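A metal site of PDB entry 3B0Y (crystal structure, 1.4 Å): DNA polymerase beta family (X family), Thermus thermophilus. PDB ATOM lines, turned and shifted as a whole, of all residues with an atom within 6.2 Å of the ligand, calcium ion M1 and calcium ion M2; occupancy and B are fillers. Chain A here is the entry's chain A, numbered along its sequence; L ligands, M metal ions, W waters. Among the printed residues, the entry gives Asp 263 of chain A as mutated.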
ATOM      1  N   ARG A 157       9.717  28.520 -14.973  1.00  0.00           N
ATOM      2  CA  ARG A 157      10.615  27.937 -13.966  1.00  0.00           C
ATOM      3  C   ARG A 157      10.282  28.541 -12.607  1.00  0.00           C
ATOM      4  O   ARG A 157       9.793  29.673 -12.510  1.00  0.00           O
ATOM      5  CB  ARG A 157      12.071  28.186 -14.365  1.00  0.00           C
ATOM      6  CG  ARG A 157      12.349  27.704 -15.797  1.00  0.00           C
ATOM      7  CD  ARG A 157      13.805  27.828 -16.198  1.00  0.00           C
ATOM      8  NE  ARG A 157      14.699  26.944 -15.437  1.00  0.00           N
ATOM      9  CZ  ARG A 157      14.903  25.657 -15.692  1.00  0.00           C
ATOM     10  NH1 ARG A 157      14.322  25.069 -16.741  1.00  0.00           N
ATOM     11  NH2 ARG A 157      15.733  24.974 -14.936  1.00  0.00           N
ATOM     12  N   CYS A 186      15.624  13.628  -8.869  1.00  0.00           N
ATOM     13  CA  CYS A 186      16.727  13.804  -9.817  1.00  0.00           C
ATOM     14  C   CYS A 186      16.569  15.115 -10.604  1.00  0.00           C
ATOM     15  O   CYS A 186      16.207  16.121 -10.007  1.00  0.00           O
ATOM     16  CB  CYS A 186      16.878  12.573 -10.708  1.00  0.00           C
ATOM     17  SG  CYS A 186      17.262  11.045  -9.787  1.00  0.00           S
ATOM     18  N   GLY A 187      16.849  15.098 -11.900  1.00  0.00           N
ATOM     19  CA  GLY A 187      16.815  16.290 -12.734  1.00  0.00           C
ATOM     20  C   GLY A 187      17.645  17.435 -12.181  1.00  0.00           C
ATOM     21  O   GLY A 187      18.602  17.278 -11.396  1.00  0.00           O
ATOM     22  N   SER A 188      17.272  18.640 -12.606  1.00  0.00           N
ATOM     23  CA  SER A 188      18.034  19.831 -12.215  1.00  0.00           C
ATOM     24  C   SER A 188      17.957  20.152 -10.733  1.00  0.00           C
ATOM     25  O   SER A 188      18.892  20.753 -10.179  1.00  0.00           O
ATOM     26  CB  SER A 188      17.595  21.032 -13.057  1.00  0.00           C
ATOM     27  OG  SER A 188      16.219  21.278 -12.781  1.00  0.00           O
ATOM     28  N   ALA A 189      16.912  19.678 -10.065  1.00  0.00           N
ATOM     29  CA  ALA A 189      16.828  19.869  -8.617  1.00  0.00           C
ATOM     30  C   ALA A 189      17.994  19.175  -7.910  1.00  0.00           C
ATOM     31  O   ALA A 189      18.568  19.697  -6.956  1.00  0.00           O
ATOM     32  CB  ALA A 189      15.513  19.323  -8.054  1.00  0.00           C
ATOM     33  N   ARG A 191      20.856  18.695  -9.035  1.00  0.00           N
ATOM     34  CA  ARG A 191      22.063  19.470  -9.367  1.00  0.00           C
ATOM     35  C   ARG A 191      22.081  20.847  -8.662  1.00  0.00           C
ATOM     36  O   ARG A 191      23.028  21.592  -8.847  1.00  0.00           O
ATOM     37  CB  ARG A 191      22.220  19.634 -10.876  1.00  0.00           C
ATOM     38  CG  ARG A 191      22.097  18.324 -11.659  1.00  0.00           C
ATOM     39  CD  ARG A 191      22.711  18.421 -13.069  1.00  0.00           C
ATOM     40  NE  ARG A 191      22.168  19.565 -13.806  1.00  0.00           N
ATOM     41  CZ  ARG A 191      21.047  19.564 -14.521  1.00  0.00           C
ATOM     42  NH1 ARG A 191      20.263  18.475 -14.613  1.00  0.00           N
ATOM     43  NH2 ARG A 191      20.661  20.677 -15.159  1.00  0.00           N
ATOM     44  N   LYS A 193      20.389  23.470  -9.235  1.00  0.00           N
ATOM     45  CA  LYS A 193      20.142  24.610 -10.129  1.00  0.00           C
ATOM     46  C   LYS A 193      19.166  25.559  -9.457  1.00  0.00           C
ATOM     47  O   LYS A 193      18.212  25.106  -8.808  1.00  0.00           O
ATOM     48  CB  LYS A 193      19.602  24.085 -11.449  1.00  0.00           C
ATOM     49  CG  LYS A 193      19.656  25.133 -12.561  1.00  0.00           C
ATOM     50  CD  LYS A 193      19.175  24.511 -13.853  1.00  0.00           C
ATOM     51  CE  LYS A 193      19.172  25.520 -14.994  1.00  0.00           C
ATOM     52  NZ  LYS A 193      20.575  25.818 -15.389  1.00  0.00           N
ATOM     53  N   THR A 195      16.839  27.613 -10.440  1.00  0.00           N
ATOM     54  CA  THR A 195      15.438  27.557 -10.910  1.00  0.00           C
ATOM     55  C   THR A 195      15.283  26.230 -11.590  1.00  0.00           C
ATOM     56  O   THR A 195      16.242  25.712 -12.189  1.00  0.00           O
ATOM     57  CB  THR A 195      15.012  28.698 -11.848  1.00  0.00           C
ATOM     58  OG1 THR A 195      15.680  28.568 -13.100  1.00  0.00           O
ATOM     59  CG2 THR A 195      15.339  30.066 -11.200  1.00  0.00           C
ATOM     60  N   VAL A 196      14.084  25.679 -11.494  1.00  0.00           N
ATOM     61  CA  VAL A 196      13.801  24.346 -12.035  1.00  0.00           C
ATOM     62  C   VAL A 196      12.566  24.358 -12.902  1.00  0.00           C
ATOM     63  O   VAL A 196      11.621  25.140 -12.656  1.00  0.00           O
ATOM     64  CB  VAL A 196      13.684  23.269 -10.940  1.00  0.00           C
ATOM     65  CG1 VAL A 196      15.031  23.168 -10.192  1.00  0.00           C
ATOM     66  CG2 VAL A 196      12.507  23.583  -9.998  1.00  0.00           C
ATOM     67  N   GLY A 197      12.550  23.487 -13.901  1.00  0.00           N
ATOM     68  CA  GLY A 197      11.320  23.213 -14.651  1.00  0.00           C
ATOM     69  C   GLY A 197      10.560  22.124 -13.918  1.00  0.00           C
ATOM     70  O   GLY A 197      10.325  22.196 -12.707  1.00  0.00           O
ATOM     71  N   ASP A 198      10.155  21.100 -14.648  1.00  0.00           N
ATOM     72  CA  ASP A 198       9.455  20.007 -13.993  1.00  0.00           C
ATOM     73  C   ASP A 198      10.375  19.262 -13.002  1.00  0.00           C
ATOM     74  O   ASP A 198      11.614  19.389 -13.069  1.00  0.00           O
ATOM     75  CB  ASP A 198       8.790  19.049 -15.007  1.00  0.00           C
ATOM     76  CG  ASP A 198       9.776  18.271 -15.845  1.00  0.00           C
ATOM     77  OD1 ASP A 198      10.976  18.173 -15.530  1.00  0.00           O
ATOM     78  OD2 ASP A 198       9.350  17.696 -16.865  1.00  0.00           O
ATOM     79  N   LEU A 199       9.757  18.511 -12.096  1.00  0.00           N
ATOM     80  CA  LEU A 199      10.508  17.696 -11.136  1.00  0.00           C
ATOM     81  C   LEU A 199      10.522  16.259 -11.623  1.00  0.00           C
ATOM     82  O   LEU A 199       9.540  15.795 -12.153  1.00  0.00           O
ATOM     83  CB  LEU A 199       9.852  17.772  -9.760  1.00  0.00           C
ATOM     84  CG  LEU A 199       9.964  19.164  -9.131  1.00  0.00           C
ATOM     85  CD1 LEU A 199       8.974  19.329  -8.018  1.00  0.00           C
ATOM     86  CD2 LEU A 199      11.362  19.497  -8.696  1.00  0.00           C
ATOM     87  N   ASP A 200      11.649  15.576 -11.444  1.00  0.00           N
ATOM     88  CA  ASP A 200      11.848  14.249 -12.023  1.00  0.00           C
ATOM     89  C   ASP A 200      12.256  13.290 -10.913  1.00  0.00           C
ATOM     90  O   ASP A 200      13.199  13.582 -10.166  1.00  0.00           O
ATOM     91  CB  ASP A 200      13.005  14.327 -13.032  1.00  0.00           C
ATOM     92  CG  ASP A 200      12.774  15.395 -14.043  1.00  0.00           C
ATOM     93  OD1 ASP A 200      12.071  15.115 -15.038  1.00  0.00           O
ATOM     94  OD2 ASP A 200      13.261  16.537 -13.818  1.00  0.00           O
ATOM     95  N   ASP A 243       7.592  14.229 -13.454  1.00  0.00           N
ATOM     96  CA  ASP A 243       7.894  13.060 -14.245  1.00  0.00           C
ATOM     97  C   ASP A 243       8.423  11.966 -13.315  1.00  0.00           C
ATOM     98  O   ASP A 243       9.225  12.229 -12.416  1.00  0.00           O
ATOM     99  CB  ASP A 243       9.003  13.367 -15.241  1.00  0.00           C
ATOM    100  CG  ASP A 243       8.555  14.213 -16.416  1.00  0.00           C
ATOM    101  OD1 ASP A 243       7.360  14.316 -16.700  1.00  0.00           O
ATOM    102  OD2 ASP A 243       9.460  14.745 -17.083  1.00  0.00           O
ATOM    103  N   GLN A 257      21.991   8.331 -12.811  1.00  0.00           N
ATOM    104  CA  GLN A 257      22.831   9.145 -13.678  1.00  0.00           C
ATOM    105  C   GLN A 257      21.970   9.710 -14.828  1.00  0.00           C
ATOM    106  O   GLN A 257      21.994  10.929 -15.131  1.00  0.00           O
ATOM    107  CB  GLN A 257      23.990   8.313 -14.198  1.00  0.00           C
ATOM    108  CG  GLN A 257      25.064   9.156 -14.895  1.00  0.00           C
ATOM    109  CD  GLN A 257      24.633   9.585 -16.298  1.00  0.00           C
ATOM    110  OE1 GLN A 257      24.162   8.784 -17.108  1.00  0.00           O
ATOM    111  NE2 GLN A 257      24.785  10.870 -16.582  1.00  0.00           N
ATOM    112  N   TYR A 258      21.190   8.839 -15.466  1.00  0.00           N
ATOM    113  CA  TYR A 258      20.393   9.243 -16.621  1.00  0.00           C
ATOM    114  C   TYR A 258      19.477  10.410 -16.258  1.00  0.00           C
ATOM    115  O   TYR A 258      19.384  11.401 -16.998  1.00  0.00           O
ATOM    116  CB  TYR A 258      19.565   8.036 -17.089  1.00  0.00           C
ATOM    117  CG  TYR A 258      18.593   8.360 -18.188  1.00  0.00           C
ATOM    118  CD1 TYR A 258      18.975   8.261 -19.517  1.00  0.00           C
ATOM    119  CD2 TYR A 258      17.312   8.801 -17.885  1.00  0.00           C
ATOM    120  CE1 TYR A 258      18.089   8.576 -20.531  1.00  0.00           C
ATOM    121  CE2 TYR A 258      16.407   9.101 -18.897  1.00  0.00           C
ATOM    122  CZ  TYR A 258      16.798   9.006 -20.209  1.00  0.00           C
ATOM    123  OH  TYR A 258      15.922   9.335 -21.221  1.00  0.00           O
ATOM    124  N   LEU A 259      18.734  10.252 -15.170  1.00  0.00           N
ATOM    125  CA  LEU A 259      17.690  11.202 -14.857  1.00  0.00           C
ATOM    126  C   LEU A 259      18.214  12.488 -14.200  1.00  0.00           C
ATOM    127  O   LEU A 259      17.469  13.453 -14.074  1.00  0.00           O
ATOM    128  CB  LEU A 259      16.605  10.508 -14.029  1.00  0.00           C
ATOM    129  CG  LEU A 259      15.266  11.251 -14.029  1.00  0.00           C
ATOM    130  CD1 LEU A 259      14.763  11.552 -15.395  1.00  0.00           C
ATOM    131  CD2 LEU A 259      14.218  10.559 -13.175  1.00  0.00           C
ATOM    132  N   THR A 260      19.468  12.462 -13.747  1.00  0.00           N
ATOM    133  CA  THR A 260      20.070  13.649 -13.130  1.00  0.00           C
ATOM    134  C   THR A 260      20.710  14.556 -14.169  1.00  0.00           C
ATOM    135  O   THR A 260      20.741  15.770 -13.998  1.00  0.00           O
ATOM    136  CB  THR A 260      21.106  13.213 -12.060  1.00  0.00           C
ATOM    137  OG1 THR A 260      20.388  12.503 -11.029  1.00  0.00           O
ATOM    138  CG2 THR A 260      21.819  14.420 -11.426  1.00  0.00           C
ATOM    139  N   GLY A 261      21.235  13.972 -15.252  1.00  0.00           N
ATOM    140  CA  GLY A 261      21.899  14.752 -16.272  1.00  0.00           C
ATOM    141  C   GLY A 261      23.021  15.593 -15.681  1.00  0.00           C
ATOM    142  O   GLY A 261      23.700  15.161 -14.758  1.00  0.00           O
ATOM    143  N   SER A 262      23.244  16.822 -16.162  1.00  0.00           N
ATOM    144  CA  SER A 262      22.559  17.424 -17.300  1.00  0.00           C
ATOM    145  C   SER A 262      22.728  16.581 -18.556  1.00  0.00           C
ATOM    146  O   SER A 262      23.586  15.673 -18.630  1.00  0.00           O
ATOM    147  CB  SER A 262      23.169  18.793 -17.536  1.00  0.00           C
ATOM    148  OG  SER A 262      24.495  18.652 -18.044  1.00  0.00           O
ATOM    149  N   ASP A 263      21.941  16.900 -19.579  1.00  0.00           N
ATOM    150  CA  ASP A 263      22.056  16.229 -20.850  1.00  0.00           C
ATOM    151  C   ASP A 263      23.509  16.341 -21.341  1.00  0.00           C
ATOM    152  O   ASP A 263      24.086  15.355 -21.802  1.00  0.00           O
ATOM    153  CB  ASP A 263      21.085  16.867 -21.844  1.00  0.00           C
ATOM    154  CG  ASP A 263      20.989  16.106 -23.144  1.00  0.00           C
ATOM    155  OD1 ASP A 263      20.963  14.863 -23.135  1.00  0.00           O
ATOM    156  OD2 ASP A 263      20.932  16.790 -24.184  1.00  0.00           O
ATOM    157  N   SER A 266      25.706  13.848 -19.559  1.00  0.00           N
ATOM    158  CA  SER A 266      25.437  12.471 -19.968  1.00  0.00           C
ATOM    159  C   SER A 266      26.008  12.215 -21.369  1.00  0.00           C
ATOM    160  O   SER A 266      26.507  11.128 -21.635  1.00  0.00           O
ATOM    161  CB  SER A 266      23.949  12.218 -19.969  1.00  0.00           C
ATOM    162  OG  SER A 266      23.447  12.326 -18.660  1.00  0.00           O
HETATM  163  P1  LIG L   1      14.778  21.487 -16.110  1.00  0.00           P
HETATM  164  O1  LIG L   1      13.614  20.535 -15.965  1.00  0.00           O
HETATM  165  O2  LIG L   1      14.724  22.368 -17.342  1.00  0.00           O
HETATM  166  O3  LIG L   1      15.013  22.291 -14.838  1.00  0.00           O
HETATM  167  O4  LIG L   1      16.132  20.595 -16.254  1.00  0.00           O
HETATM  168  P2  LIG L   1      16.330  19.016 -16.152  1.00  0.00           P
HETATM  169  O5  LIG L   1      17.785  18.739 -16.241  1.00  0.00           O
HETATM  170  O6  LIG L   1      15.545  18.439 -14.991  1.00  0.00           O
HETATM  171  O7  LIG L   1      15.704  18.472 -17.526  1.00  0.00           O
HETATM  172  P3  LIG L   1      14.493  17.495 -17.930  1.00  0.00           P
HETATM  173  O8  LIG L   1      13.439  17.482 -16.865  1.00  0.00           O
HETATM  174  O9  LIG L   1      14.099  17.894 -19.322  1.00  0.00           O
HETATM  175  O10 LIG L   1      15.183  16.090 -18.054  1.00  0.00           O
HETATM  176  C1  LIG L   1      15.643  15.425 -16.861  1.00  0.00           C
HETATM  177  C2  LIG L   1      16.945  14.699 -17.160  1.00  0.00           C
HETATM  178  O11 LIG L   1      16.669  13.719 -18.156  1.00  0.00           O
HETATM  179  C3  LIG L   1      18.059  15.552 -17.765  1.00  0.00           C
HETATM  180  O12 LIG L   1      18.857  16.198 -16.788  1.00  0.00           O
HETATM  181  C4  LIG L   1      18.905  14.528 -18.522  1.00  0.00           C
HETATM  182  C5  LIG L   1      17.880  13.446 -18.906  1.00  0.00           C
HETATM  183  N1  LIG L   1      17.568  13.507 -20.347  1.00  0.00           N
HETATM  184  C6  LIG L   1      17.295  12.458 -21.140  1.00  0.00           C
HETATM  185  N2  LIG L   1      17.041  12.877 -22.403  1.00  0.00           N
HETATM  186  C7  LIG L   1      17.154  14.213 -22.435  1.00  0.00           C
HETATM  187  C8  LIG L   1      17.023  15.286 -23.454  1.00  0.00           C
HETATM  188  O13 LIG L   1      16.722  15.016 -24.643  1.00  0.00           O
HETATM  189  N3  LIG L   1      17.236  16.562 -23.071  1.00  0.00           N
HETATM  190  C9  LIG L   1      17.555  16.909 -21.808  1.00  0.00           C
HETATM  191  N4  LIG L   1      17.765  18.220 -21.478  1.00  0.00           N
HETATM  192  N5  LIG L   1      17.687  15.965 -20.845  1.00  0.00           N
HETATM  193  C10 LIG L   1      17.503  14.640 -21.092  1.00  0.00           C
HETATM  194 CA    CA M   1      11.303  16.191 -17.008  1.00  0.00          CA
HETATM  195 CA    CA M   2      13.188  18.624 -14.746  1.00  0.00          CA
HETATM  196  O   HOH W   1      13.769  22.237 -19.868  1.00  0.00           O
HETATM  197  O   HOH W   2      12.369  14.364 -18.177  1.00  0.00           O
HETATM  198  O   HOH W   3      19.215  20.813 -17.514  1.00  0.00           O
HETATM  199  O   HOH W   4      11.238  17.074 -19.246  1.00  0.00           O
HETATM  200  O   HOH W   5      14.187  19.493 -12.586  1.00  0.00           O
HETATM  201  O   HOH W   6      20.114  19.067 -19.486  1.00  0.00           O
HETATM  202  O   HOH W   7      17.371  23.036 -18.136  1.00  0.00           O
HETATM  203  O   HOH W   8      11.325  20.956 -17.397  1.00  0.00           O
HETATM  204  O   HOH W   9      20.874  11.810 -19.199  1.00  0.00           O
HETATM  205  O   HOH W  10      14.398  13.674 -19.954  1.00  0.00           O
HETATM  206  O   HOH W  11      14.137  16.042 -21.435  1.00  0.00           O
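Water W3 bridges the guanidinium group of Arg 191 (2.8 Å) and an oxygen (O5) of the ligand (2.8 Å).
Water W6 lies within hydrogen-bond range of the backbone NH (N) of Asp 263 (2.8 Å) and a nitrogen (N4) of the ligand (3.2 Å).
Water W9 bridges OG of Ser 266 (2.7 Å) and O of Tyr 258 (2.7 Å).
Calcium ion M1 is bound by the side-chain carboxylate (OD2) of Asp 243 (2.3 Å), the side-chain carboxylate (OD1) of Asp 200 (2.4 Å), water W4 (2.4 Å), water W2 (2.4 Å), the side-chain carboxylate (OD2) of Asp 198 (2.5 Å), the side-chain carboxylate (OD1) of Asp 198 (2.5 Å) and an oxygen (O8) of the ligand (2.5 Å).
Calcium ion M1 has seven donor atoms within binding distance.
Calcium ion M2 is bound by OD2 of Asp 200, O1 of the ligand, O6 of the ligand, OD1 of Asp 198, O8 of the ligand, O of Asp 198 and water W5.
The backbone NH (N) of Ser 188 lies close to an oxygen (O6) of the ligand (3.0 Å).
An oxygen (O3) of the ligand lies within hydrogen-bond range of the side-chain hydroxyl of Ser 188.
The guanidinium group (NH2) of Arg 157 lies within salt-bridge range of an oxygen (O3) of the ligand, at 2.8 Å.
N of Gly 197 lies within hydrogen-bond range of O3 of the ligand, 2.9 Å away.
O5 of the ligand is in salt-bridge range of NH1 of Arg 191 (3.0 Å).
The backbone carbonyl oxygen (O) of Thr 260 lies within hydrogen-bond range of an oxygen (O12) of the ligand (3.4 Å).
Of the 22 residues printed, 3 come within 4 Å of calcium ion M1.
The backbone carbonyl oxygen (O) of Asp 200 lies within hydrogen-bond range of the backbone NH (N) of Cys 186.
O of Leu 199 lies within hydrogen-bond range of N of Asp 243 (2.8 Å).
N of Lys 193 is in hydrogen-bond range of O of Ser 188, at 3.2 Å.
NH2 of Arg 157 lies within hydrogen-bond range of O of Thr 195, 2.9 Å away.
The guanidinium group (NH1) of Arg 191 is in hydrogen-bond range of the backbone carbonyl oxygen (O) of Thr 260, 2.8 Å away.
The backbone carbonyl oxygen of Leu 259 is in hydrogen-bond range of the backbone NH of Gly 187.
The side-chain hydroxyl (OG1) of Thr 260 lies close to the side-chain sulfur (SG) of Cys 186.
The side-chain hydroxyl (OG) of Ser 266 lies within hydrogen-bond range of the backbone carbonyl oxygen (O) of Ser 262 (3.4 Å).
Gly 187 touches the ligand.
CA of Val 196 touches O3 of the ligand, at 3.7 Å.
Tyr 258 touches the ligand (O to C5, 3.2 Å).
Leu 259 touches the ligand.
CA of Gly 261 touches O12 of the ligand, 3.4 Å away.
CA of Ser 262 touches O12 of the ligand (3.9 Å).
Asp 263 touches the ligand.
Hydrophobic or aromatic side chains that line the ligand: Tyr 258 and Leu 259.
Within 4 Å of the ligand: Arg 157, Gly 187, Ser 188, Arg 191, Val 196, Gly 197, Asp 198, Asp 200, Tyr 258, Leu 259, Thr 260, Gly 261, Ser 262 and Asp 263.
Two residues have an atom within 4 Å of calcium ion M2: Asp 198 and Asp 200.
The nearest printed residue that does not touch calcium ion M2 is Leu 199 (4.3 Å).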
